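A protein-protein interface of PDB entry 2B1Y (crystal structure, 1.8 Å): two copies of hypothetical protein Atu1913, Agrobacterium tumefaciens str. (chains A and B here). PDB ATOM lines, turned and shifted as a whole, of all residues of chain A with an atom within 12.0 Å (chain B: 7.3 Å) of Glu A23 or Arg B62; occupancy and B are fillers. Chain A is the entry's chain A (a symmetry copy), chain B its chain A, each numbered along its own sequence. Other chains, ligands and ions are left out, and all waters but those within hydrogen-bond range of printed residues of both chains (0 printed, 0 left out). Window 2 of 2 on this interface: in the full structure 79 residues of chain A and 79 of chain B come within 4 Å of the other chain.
The backbone NH (N) of Ile A24 sits at hydrogen-bond distance from the backbone carbonyl oxygen (O) of Ile B61 (2.7 Å).
The side-chain carboxylate (OE2) of Glu A23 is in salt-bridge range of the guanidinium group (NE) of Arg B62.
The backbone carbonyl oxygen (O) of Ile B63 sits at hydrogen-bond distance from the backbone NH (N) of Leu A22.
The backbone carbonyl oxygen (O) of Leu B73 sits at hydrogen-bond distance from the backbone NH (N) of Tyr A11 (2.8 Å).
O of Ser B87 sits at hydrogen-bond distance from N of Ser A25.
The backbone NH of Glu A23 sits at hydrogen-bond distance from the backbone carbonyl oxygen of Lys B89.
N of Leu B91 is in hydrogen-bond range of O of Thr A21 (2.8 Å).
The backbone carbonyl oxygen (O) of Leu A22 sits close to the backbone carbonyl oxygen (O) of Ile B61 (3.5 Å).
The backbone carbonyl oxygen (O) of Arg A17 is in hydrogen-bond range of the side-chain hydroxyl (OG1) of Thr A20 (2.8 Å).
O of Gly A19 is in hydrogen-bond range of OG1 of Thr A21 (3.2 Å).
Among the printed residues, pairs that only touch across the chains: Thr A9 with Leu B73 (3.7 Å), Tyr A11 with Ser B87 (3.8 Å), Tyr A11 with Val B88 (3.5 Å), Leu A16 with Met B90 (3.97 Å), Thr A20 with Ala B64 (3.5 Å), Thr A20 with Leu B91 (3.4 Å), Thr A21 with Arg B62 (3.9 Å), Thr A21 with Ile B63 (3.6 Å), Thr A21 with Lys B89 (3.7 Å), Thr A21 with Met B90 (3.8 Å), Leu A22 with Arg B62 (3.2 Å), Leu A22 with Lys B89 (3.6 Å), Glu A23 with Pro B60 (3.98 Å), Glu A23 with Ile B61 (3.4 Å), Glu A23 with Ser B87 (3.8 Å), Glu A23 with Val B88 (3.4 Å), Glu A23 with Leu B91 (3.999 Å), Ile A24 with Pro B60 (3.1 Å), Ile A24 with Ile B63 (3.8 Å), Ile A24 with Leu B73 (3.9 Å), Ile A24 with Ser B87 (3.4 Å), Ile A24 with Val B88 (3.9 Å), Ser A25 with Pro B60 (3.9 Å), Val A32 with Ile B63 (3.7 Å), Val A32 with Leu B73 (3.9 Å), Arg A33 with Leu B73 (3.5 Å) and Leu A34 with Ile B63 (3.7 Å).
Arg B62 touches just these residues of chain A: Thr A21, Leu A22 and Glu A23.
Of chain A, only Leu A22 (3.5 Å), Glu A23 (3.4 Å) and Ile A24 (2.7 Å) come within 4 Å of Ile B61.
Ala B64 touches just one residue of chain A: Thr A20 (3.5 Å).
Of chain A, only Tyr A11 (3.8 Å), Glu A23 (3.8 Å), Ile A24 (3.4 Å) and Ser A25 (2.8 Å) come within 4 Å of Ser B87.
Of chain A, only Thr A21 (3.7 Å), Leu A22 (3.6 Å) and Glu A23 (2.8 Å) come within 4 Å of Lys B89.
Printed residues of chain A within 4 Å of Leu B91: Thr A20 (3.4 Å), Thr A21 (2.8 Å) and Glu A23 (3.999 Å).
Printed residues of chain B within 4 Å of Arg A33: Leu B73.
Printed residues of chain B within 4 Å of Ile A24: Pro B60, Ile B61, Ile B63, Leu B73, Ser B87 and Val B88.
Ser A27 touches none of the printed residues of chain B.
The nearest printed residue of chain B that does not touch Glu A23 is Met B90 (5.0 Å).
The nearest printed residue of chain B that does not touch Leu A22 is Met B90 (4.04 Å).
Of the 19 printed residues of chain A, 12 touch a printed residue of chain B.
Hydrophobic or aromatic side chains of chain B that line the printed part of chain A: Pro B60, Ile B61, Ile B63, Leu B73, Val B88, Met B90 and Leu B91.
Among the printed residues, 35 pairs touch across the chains.
Among the printed residues, Asp or Glu carboxylates within 4 Å of a Lys or Arg side-chain nitrogen of the other chain: Glu A23 with Arg B62 (3.2 Å).
No position is printed for both chains.
Of the 35 pairs that touch across the chains among the printed residues, none has its exchanged pair printed and touching as well.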
ATOM      1  N   THR A   9     -28.655  40.181 -25.647  1.00  0.00           N
ATOM      2  CA  THR A   9     -28.171  39.620 -26.876  1.00  0.00           C
ATOM      3  C   THR A   9     -28.890  38.299 -27.096  1.00  0.00           C
ATOM      4  O   THR A   9     -28.990  37.509 -26.177  1.00  0.00           O
ATOM      5  CB  THR A   9     -26.683  39.264 -26.738  1.00  0.00           C
ATOM      6  OG1 THR A   9     -25.935  40.457 -26.502  1.00  0.00           O
ATOM      7  CG2 THR A   9     -26.196  38.580 -28.014  1.00  0.00           C
ATOM      8  N   TYR A  11     -29.112  34.790 -29.264  1.00  0.00           N
ATOM      9  CA  TYR A  11     -28.660  33.775 -30.232  1.00  0.00           C
ATOM     10  C   TYR A  11     -29.829  32.823 -30.531  1.00  0.00           C
ATOM     11  O   TYR A  11     -30.328  32.143 -29.637  1.00  0.00           O
ATOM     12  CB  TYR A  11     -27.453  32.945 -29.712  1.00  0.00           C
ATOM     13  CG  TYR A  11     -26.270  33.773 -29.259  1.00  0.00           C
ATOM     14  CD1 TYR A  11     -25.207  34.017 -30.134  1.00  0.00           C
ATOM     15  CD2 TYR A  11     -26.214  34.325 -27.967  1.00  0.00           C
ATOM     16  CE1 TYR A  11     -24.100  34.795 -29.766  1.00  0.00           C
ATOM     17  CE2 TYR A  11     -25.078  35.136 -27.574  1.00  0.00           C
ATOM     18  CZ  TYR A  11     -24.041  35.349 -28.504  1.00  0.00           C
ATOM     19  OH  TYR A  11     -22.955  36.120 -28.181  1.00  0.00           O
ATOM     20  N   LEU A  13     -30.404  29.528 -31.758  1.00  0.00           N
ATOM     21  CA  LEU A  13     -29.568  28.339 -31.954  1.00  0.00           C
ATOM     22  C   LEU A  13     -30.203  27.260 -32.831  1.00  0.00           C
ATOM     23  O   LEU A  13     -29.572  26.230 -33.092  1.00  0.00           O
ATOM     24  CB  LEU A  13     -29.187  27.711 -30.600  1.00  0.00           C
ATOM     25  CG  LEU A  13     -28.471  28.660 -29.624  1.00  0.00           C
ATOM     26  CD1 LEU A  13     -28.163  27.919 -28.349  1.00  0.00           C
ATOM     27  CD2 LEU A  13     -27.193  29.200 -30.224  1.00  0.00           C
ATOM     28  N   LEU A  16     -31.666  21.884 -31.731  1.00  0.00           N
ATOM     29  CA  LEU A  16     -30.555  21.160 -31.133  1.00  0.00           C
ATOM     30  C   LEU A  16     -31.055  19.886 -30.462  1.00  0.00           C
ATOM     31  O   LEU A  16     -32.107  19.907 -29.835  1.00  0.00           O
ATOM     32  CB  LEU A  16     -29.863  22.022 -30.070  1.00  0.00           C
ATOM     33  CG  LEU A  16     -29.330  23.392 -30.512  1.00  0.00           C
ATOM     34  CD1 LEU A  16     -28.797  24.159 -29.300  1.00  0.00           C
ATOM     35  CD2 LEU A  16     -28.245  23.261 -31.589  1.00  0.00           C
ATOM     36  N   ARG A  17     -30.275  18.813 -30.574  1.00  0.00           N
ATOM     37  CA  ARG A  17     -30.616  17.537 -29.960  1.00  0.00           C
ATOM     38  C   ARG A  17     -30.358  17.605 -28.463  1.00  0.00           C
ATOM     39  O   ARG A  17     -29.408  18.266 -28.024  1.00  0.00           O
ATOM     40  CB  ARG A  17     -29.783  16.404 -30.577  1.00  0.00           C
ATOM     41  CG  ARG A  17     -30.521  15.064 -30.619  1.00  0.00           C
ATOM     42  CD  ARG A  17     -29.578  13.879 -30.781  1.00  0.00           C
ATOM     43  NE  ARG A  17     -30.282  12.614 -30.555  1.00  0.00           N
ATOM     44  CZ  ARG A  17     -29.814  11.407 -30.879  1.00  0.00           C
ATOM     45  NH1 ARG A  17     -28.628  11.268 -31.448  1.00  0.00           N
ATOM     46  NH2 ARG A  17     -30.540  10.334 -30.630  1.00  0.00           N
ATOM     47  N   GLY A  19     -28.864  17.065 -25.002  1.00  0.00           N
ATOM     48  CA  GLY A  19     -27.463  16.787 -24.672  1.00  0.00           C
ATOM     49  C   GLY A  19     -26.419  17.668 -25.354  1.00  0.00           C
ATOM     50  O   GLY A  19     -25.264  17.729 -24.906  1.00  0.00           O
ATOM     51  N   THR A  20     -26.796  18.360 -26.418  1.00  0.00           N
ATOM     52  CA  THR A  20     -25.911  19.389 -26.976  1.00  0.00           C
ATOM     53  C   THR A  20     -25.502  20.328 -25.841  1.00  0.00           C
ATOM     54  O   THR A  20     -26.348  20.709 -25.032  1.00  0.00           O
ATOM     55  CB  THR A  20     -26.599  20.178 -28.069  1.00  0.00           C
ATOM     56  OG1 THR A  20     -27.012  19.272 -29.099  1.00  0.00           O
ATOM     57  CG2 THR A  20     -25.659  21.250 -28.663  1.00  0.00           C
ATOM     58  N   THR A  21     -24.212  20.673 -25.790  1.00  0.00           N
ATOM     59  CA  THR A  21     -23.663  21.471 -24.692  1.00  0.00           C
ATOM     60  C   THR A  21     -23.253  22.826 -25.222  1.00  0.00           C
ATOM     61  O   THR A  21     -22.484  22.925 -26.180  1.00  0.00           O
ATOM     62  CB  THR A  21     -22.521  20.725 -23.953  1.00  0.00           C
ATOM     63  OG1 THR A  21     -23.049  19.513 -23.388  1.00  0.00           O
ATOM     64  CG2 THR A  21     -21.961  21.577 -22.814  1.00  0.00           C
ATOM     65  N   LEU A  22     -23.789  23.876 -24.613  1.00  0.00           N
ATOM     66  CA  LEU A  22     -23.425  25.207 -25.023  1.00  0.00           C
ATOM     67  C   LEU A  22     -22.315  25.703 -24.099  1.00  0.00           C
ATOM     68  O   LEU A  22     -22.475  25.712 -22.858  1.00  0.00           O
ATOM     69  CB  LEU A  22     -24.633  26.124 -24.914  1.00  0.00           C
ATOM     70  CG  LEU A  22     -25.923  25.632 -25.564  1.00  0.00           C
ATOM     71  CD1 LEU A  22     -27.021  26.686 -25.366  1.00  0.00           C
ATOM     72  CD2 LEU A  22     -25.664  25.348 -27.027  1.00  0.00           C
ATOM     73  N   GLU A  23     -21.196  26.097 -24.701  1.00  0.00           N
ATOM     74  CA  GLU A  23     -20.124  26.710 -23.955  1.00  0.00           C
ATOM     75  C   GLU A  23     -20.174  28.238 -24.104  1.00  0.00           C
ATOM     76  O   GLU A  23     -19.946  28.794 -25.200  1.00  0.00           O
ATOM     77  CB  GLU A  23     -18.769  26.135 -24.417  1.00  0.00           C
ATOM     78  CG  GLU A  23     -17.584  26.737 -23.635  1.00  0.00           C
ATOM     79  CD  GLU A  23     -16.315  25.936 -23.789  1.00  0.00           C
ATOM     80  OE1 GLU A  23     -15.659  26.068 -24.822  1.00  0.00           O
ATOM     81  OE2 GLU A  23     -15.975  25.158 -22.876  1.00  0.00           O
ATOM     82  N   ILE A  24     -20.481  28.938 -23.015  1.00  0.00           N
ATOM     83  CA  ILE A  24     -20.843  30.346 -23.147  1.00  0.00           C
ATOM     84  C   ILE A  24     -19.820  31.220 -22.441  1.00  0.00           C
ATOM     85  O   ILE A  24     -19.548  30.964 -21.253  1.00  0.00           O
ATOM     86  CB  ILE A  24     -22.260  30.581 -22.523  1.00  0.00           C
ATOM     87  CG1 ILE A  24     -23.293  29.659 -23.194  1.00  0.00           C
ATOM     88  CG2 ILE A  24     -22.648  32.065 -22.565  1.00  0.00           C
ATOM     89  CD1 ILE A  24     -24.458  29.369 -22.306  1.00  0.00           C
ATOM     90  N   SER A  25     -19.225  32.194 -23.158  1.00  0.00           N
ATOM     91  CA  SER A  25     -18.217  33.082 -22.580  1.00  0.00           C
ATOM     92  C   SER A  25     -18.848  34.447 -22.352  1.00  0.00           C
ATOM     93  O   SER A  25     -19.653  34.888 -23.182  1.00  0.00           O
ATOM     94  CB  SER A  25     -17.013  33.265 -23.531  1.00  0.00           C
ATOM     95  OG  SER A  25     -16.290  32.023 -23.759  1.00  0.00           O
ATOM     96  N   LEU A  26     -18.451  35.145 -21.291  1.00  0.00           N
ATOM     97  CA  LEU A  26     -18.990  36.477 -20.982  1.00  0.00           C
ATOM     98  C   LEU A  26     -17.918  37.342 -20.440  1.00  0.00           C
ATOM     99  O   LEU A  26     -17.044  36.834 -19.755  1.00  0.00           O
ATOM    100  CB  LEU A  26     -20.025  36.423 -19.871  1.00  0.00           C
ATOM    101  CG  LEU A  26     -21.229  35.580 -20.069  1.00  0.00           C
ATOM    102  CD1 LEU A  26     -21.872  35.428 -18.711  1.00  0.00           C
ATOM    103  CD2 LEU A  26     -22.127  36.318 -20.983  1.00  0.00           C
ATOM    104  N   SER A  27     -18.017  38.645 -20.690  1.00  0.00           N
ATOM    105  CA  SER A  27     -16.981  39.572 -20.235  1.00  0.00           C
ATOM    106  C   SER A  27     -17.183  40.061 -18.787  1.00  0.00           C
ATOM    107  O   SER A  27     -16.223  40.446 -18.112  1.00  0.00           O
ATOM    108  CB  SER A  27     -16.893  40.754 -21.191  1.00  0.00           C
ATOM    109  OG  SER A  27     -18.088  41.498 -21.114  1.00  0.00           O
ATOM    110  N   ASN A  30     -23.540  38.847 -15.851  1.00  0.00           N
ATOM    111  CA  ASN A  30     -24.792  39.028 -16.580  1.00  0.00           C
ATOM    112  C   ASN A  30     -25.633  37.772 -16.428  1.00  0.00           C
ATOM    113  O   ASN A  30     -25.177  36.775 -15.851  1.00  0.00           O
ATOM    114  CB  ASN A  30     -24.552  39.287 -18.077  1.00  0.00           C
ATOM    115  CG  ASN A  30     -24.694  40.744 -18.467  1.00  0.00           C
ATOM    116  OD1 ASN A  30     -24.537  41.674 -17.651  1.00  0.00           O
ATOM    117  ND2 ASN A  30     -24.963  40.961 -19.739  1.00  0.00           N
ATOM    118  N   ASN A  31     -26.861  37.827 -16.930  1.00  0.00           N
ATOM    119  CA  ASN A  31     -27.750  36.666 -16.867  1.00  0.00           C
ATOM    120  C   ASN A  31     -27.601  35.858 -18.139  1.00  0.00           C
ATOM    121  O   ASN A  31     -27.412  36.420 -19.221  1.00  0.00           O
ATOM    122  CB  ASN A  31     -29.217  37.112 -16.771  1.00  0.00           C
ATOM    123  CG  ASN A  31     -29.441  38.069 -15.608  1.00  0.00           C
ATOM    124  OD1 ASN A  31     -28.953  37.828 -14.507  1.00  0.00           O
ATOM    125  ND2 ASN A  31     -30.132  39.152 -15.863  1.00  0.00           N
ATOM    126  N   VAL A  32     -27.731  34.550 -17.995  1.00  0.00           N
ATOM    127  CA  VAL A  32     -27.665  33.661 -19.140  1.00  0.00           C
ATOM    128  C   VAL A  32     -28.910  32.800 -19.076  1.00  0.00           C
ATOM    129  O   VAL A  32     -29.156  32.164 -18.060  1.00  0.00           O
ATOM    130  CB  VAL A  32     -26.388  32.769 -19.053  1.00  0.00           C
ATOM    131  CG1 VAL A  32     -26.355  31.679 -20.185  1.00  0.00           C
ATOM    132  CG2 VAL A  32     -25.162  33.620 -19.129  1.00  0.00           C
ATOM    133  N   ARG A  33     -29.689  32.765 -20.152  1.00  0.00           N
ATOM    134  CA  ARG A  33     -30.972  32.048 -20.105  1.00  0.00           C
ATOM    135  C   ARG A  33     -31.106  31.279 -21.407  1.00  0.00           C
ATOM    136  O   ARG A  33     -31.102  31.886 -22.481  1.00  0.00           O
ATOM    137  CB  ARG A  33     -32.137  33.036 -20.010  1.00  0.00           C
ATOM    138  CG  ARG A  33     -31.942  34.213 -19.086  1.00  0.00           C
ATOM    139  CD  ARG A  33     -33.260  34.972 -18.930  1.00  0.00           C
ATOM    140  NE  ARG A  33     -33.054  36.349 -18.506  1.00  0.00           N
ATOM    141  CZ  ARG A  33     -33.886  37.052 -17.745  1.00  0.00           C
ATOM    142  NH1 ARG A  33     -33.578  38.316 -17.460  1.00  0.00           N
ATOM    143  NH2 ARG A  33     -34.996  36.498 -17.253  1.00  0.00           N
ATOM    144  N   LEU A  34     -31.258  29.961 -21.309  1.00  0.00           N
ATOM    145  CA  LEU A  34     -31.501  29.103 -22.425  1.00  0.00           C
ATOM    146  C   LEU A  34     -33.006  28.782 -22.413  1.00  0.00           C
ATOM    147  O   LEU A  34     -33.525  28.373 -21.377  1.00  0.00           O
ATOM    148  CB  LEU A  34     -30.690  27.817 -22.227  1.00  0.00           C
ATOM    149  CG  LEU A  34     -30.990  26.722 -23.265  1.00  0.00           C
ATOM    150  CD1 LEU A  34     -30.503  27.132 -24.680  1.00  0.00           C
ATOM    151  CD2 LEU A  34     -30.364  25.370 -22.819  1.00  0.00           C
ATOM    152  N   PRO B  60     -15.777  30.432 -19.005  1.00  0.00           N
ATOM    153  CA  PRO B  60     -17.079  30.205 -19.603  1.00  0.00           C
ATOM    154  C   PRO B  60     -17.890  29.270 -18.737  1.00  0.00           C
ATOM    155  O   PRO B  60     -17.353  28.635 -17.834  1.00  0.00           O
ATOM    156  CB  PRO B  60     -16.713  29.461 -20.866  1.00  0.00           C
ATOM    157  CG  PRO B  60     -15.498  28.737 -20.477  1.00  0.00           C
ATOM    158  CD  PRO B  60     -14.761  29.537 -19.589  1.00  0.00           C
ATOM    159  N   ILE B  61     -19.188  29.181 -19.035  1.00  0.00           N
ATOM    160  CA  ILE B  61     -20.021  28.211 -18.356  1.00  0.00           C
ATOM    161  C   ILE B  61     -20.563  27.271 -19.433  1.00  0.00           C
ATOM    162  O   ILE B  61     -20.489  27.573 -20.662  1.00  0.00           O
ATOM    163  CB  ILE B  61     -21.153  28.870 -17.587  1.00  0.00           C
ATOM    164  CG1 ILE B  61     -21.978  29.784 -18.492  1.00  0.00           C
ATOM    165  CG2 ILE B  61     -20.629  29.674 -16.344  1.00  0.00           C
ATOM    166  CD1 ILE B  61     -23.461  29.680 -18.201  1.00  0.00           C
ATOM    167  N   ARG B  62     -21.061  26.136 -18.961  1.00  0.00           N
ATOM    168  CA  ARG B  62     -21.640  25.133 -19.835  1.00  0.00           C
ATOM    169  C   ARG B  62     -23.063  24.870 -19.379  1.00  0.00           C
ATOM    170  O   ARG B  62     -23.353  24.813 -18.169  1.00  0.00           O
ATOM    171  CB  ARG B  62     -20.813  23.849 -19.835  1.00  0.00           C
ATOM    172  CG  ARG B  62     -19.482  23.979 -20.587  1.00  0.00           C
ATOM    173  CD  ARG B  62     -18.603  22.761 -20.435  1.00  0.00           C
ATOM    174  NE  ARG B  62     -17.483  22.812 -21.381  1.00  0.00           N
ATOM    175  CZ  ARG B  62     -16.623  21.822 -21.611  1.00  0.00           C
ATOM    176  NH1 ARG B  62     -15.656  21.988 -22.501  1.00  0.00           N
ATOM    177  NH2 ARG B  62     -16.719  20.666 -20.966  1.00  0.00           N
ATOM    178  N   ILE B  63     -23.946  24.740 -20.359  1.00  0.00           N
ATOM    179  CA  ILE B  63     -25.348  24.443 -20.111  1.00  0.00           C
ATOM    180  C   ILE B  63     -25.691  23.370 -21.141  1.00  0.00           C
ATOM    181  O   ILE B  63     -25.380  23.518 -22.317  1.00  0.00           O
ATOM    182  CB  ILE B  63     -26.288  25.666 -20.374  1.00  0.00           C
ATOM    183  CG1 ILE B  63     -25.940  26.878 -19.513  1.00  0.00           C
ATOM    184  CG2 ILE B  63     -27.795  25.270 -20.129  1.00  0.00           C
ATOM    185  CD1 ILE B  63     -26.934  28.069 -19.680  1.00  0.00           C
ATOM    186  N   ALA B  64     -26.310  22.276 -20.706  1.00  0.00           N
ATOM    187  CA  ALA B  64     -26.644  21.199 -21.625  1.00  0.00           C
ATOM    188  C   ALA B  64     -28.121  21.321 -21.972  1.00  0.00           C
ATOM    189  O   ALA B  64     -28.949  21.617 -21.107  1.00  0.00           O
ATOM    190  CB  ALA B  64     -26.354  19.850 -20.980  1.00  0.00           C
ATOM    191  N   LEU B  73     -30.721  31.365 -26.905  1.00  0.00           N
ATOM    192  CA  LEU B  73     -29.876  31.696 -25.767  1.00  0.00           C
ATOM    193  C   LEU B  73     -29.907  33.206 -25.630  1.00  0.00           C
ATOM    194  O   LEU B  73     -29.616  33.928 -26.613  1.00  0.00           O
ATOM    195  CB  LEU B  73     -28.439  31.227 -26.004  1.00  0.00           C
ATOM    196  CG  LEU B  73     -27.485  31.636 -24.879  1.00  0.00           C
ATOM    197  CD1 LEU B  73     -27.865  30.825 -23.656  1.00  0.00           C
ATOM    198  CD2 LEU B  73     -26.067  31.408 -25.306  1.00  0.00           C
ATOM    199  N   SER B  87     -19.915  35.137 -26.191  1.00  0.00           N
ATOM    200  CA  SER B  87     -19.757  34.205 -27.305  1.00  0.00           C
ATOM    201  C   SER B  87     -20.326  32.870 -26.868  1.00  0.00           C
ATOM    202  O   SER B  87     -20.425  32.578 -25.657  1.00  0.00           O
ATOM    203  CB  SER B  87     -18.302  34.126 -27.781  1.00  0.00           C
ATOM    204  OG  SER B  87     -17.518  33.415 -26.849  1.00  0.00           O
ATOM    205  N   VAL B  88     -20.768  32.076 -27.841  1.00  0.00           N
ATOM    206  CA  VAL B  88     -21.308  30.754 -27.570  1.00  0.00           C
ATOM    207  C   VAL B  88     -20.736  29.726 -28.578  1.00  0.00           C
ATOM    208  O   VAL B  88     -20.684  29.975 -29.785  1.00  0.00           O
ATOM    209  CB  VAL B  88     -22.886  30.732 -27.497  1.00  0.00           C
ATOM    210  CG1 VAL B  88     -23.536  31.213 -28.768  1.00  0.00           C
ATOM    211  CG2 VAL B  88     -23.404  29.321 -27.109  1.00  0.00           C
ATOM    212  N   LYS B  89     -20.273  28.594 -28.062  1.00  0.00           N
ATOM    213  CA  LYS B  89     -19.715  27.522 -28.887  1.00  0.00           C
ATOM    214  C   LYS B  89     -20.618  26.343 -28.608  1.00  0.00           C
ATOM    215  O   LYS B  89     -20.902  26.023 -27.454  1.00  0.00           O
ATOM    216  CB  LYS B  89     -18.257  27.235 -28.494  1.00  0.00           C
ATOM    217  CG  LYS B  89     -17.515  26.293 -29.395  1.00  0.00           C
ATOM    218  CD  LYS B  89     -16.108  26.016 -28.860  1.00  0.00           C
ATOM    219  CE  LYS B  89     -15.111  25.992 -30.017  1.00  0.00           C
ATOM    220  NZ  LYS B  89     -13.902  25.083 -29.868  1.00  0.00           N
ATOM    221  N   MET B  90     -21.080  25.712 -29.685  1.00  0.00           N
ATOM    222  CA  MET B  90     -22.029  24.631 -29.594  1.00  0.00           C
ATOM    223  C   MET B  90     -21.225  23.327 -29.709  1.00  0.00           C
ATOM    224  O   MET B  90     -20.617  23.033 -30.772  1.00  0.00           O
ATOM    225  CB  MET B  90     -23.108  24.776 -30.687  1.00  0.00           C
ATOM    226  CG  MET B  90     -23.981  26.113 -30.622  1.00  0.00           C
ATOM    227  SD  MET B  90     -25.336  25.922 -32.035  1.00  0.00           S
ATOM    228  CE  MET B  90     -24.151  25.841 -33.561  1.00  0.00           C
ATOM    229  N   LEU B  91     -21.148  22.607 -28.589  1.00  0.00           N
ATOM    230  CA  LEU B  91     -20.387  21.363 -28.503  1.00  0.00           C
ATOM    231  C   LEU B  91     -21.322  20.156 -28.733  1.00  0.00           C
ATOM    232  O   LEU B  91     -22.464  20.124 -28.237  1.00  0.00           O
ATOM    233  CB  LEU B  91     -19.662  21.250 -27.148  1.00  0.00           C
ATOM    234  CG  LEU B  91     -18.867  22.471 -26.590  1.00  0.00           C
ATOM    235  CD1 LEU B  91     -18.392  22.227 -25.179  1.00  0.00           C
ATOM    236  CD2 LEU B  91     -17.679  22.872 -27.460  1.00  0.00           C
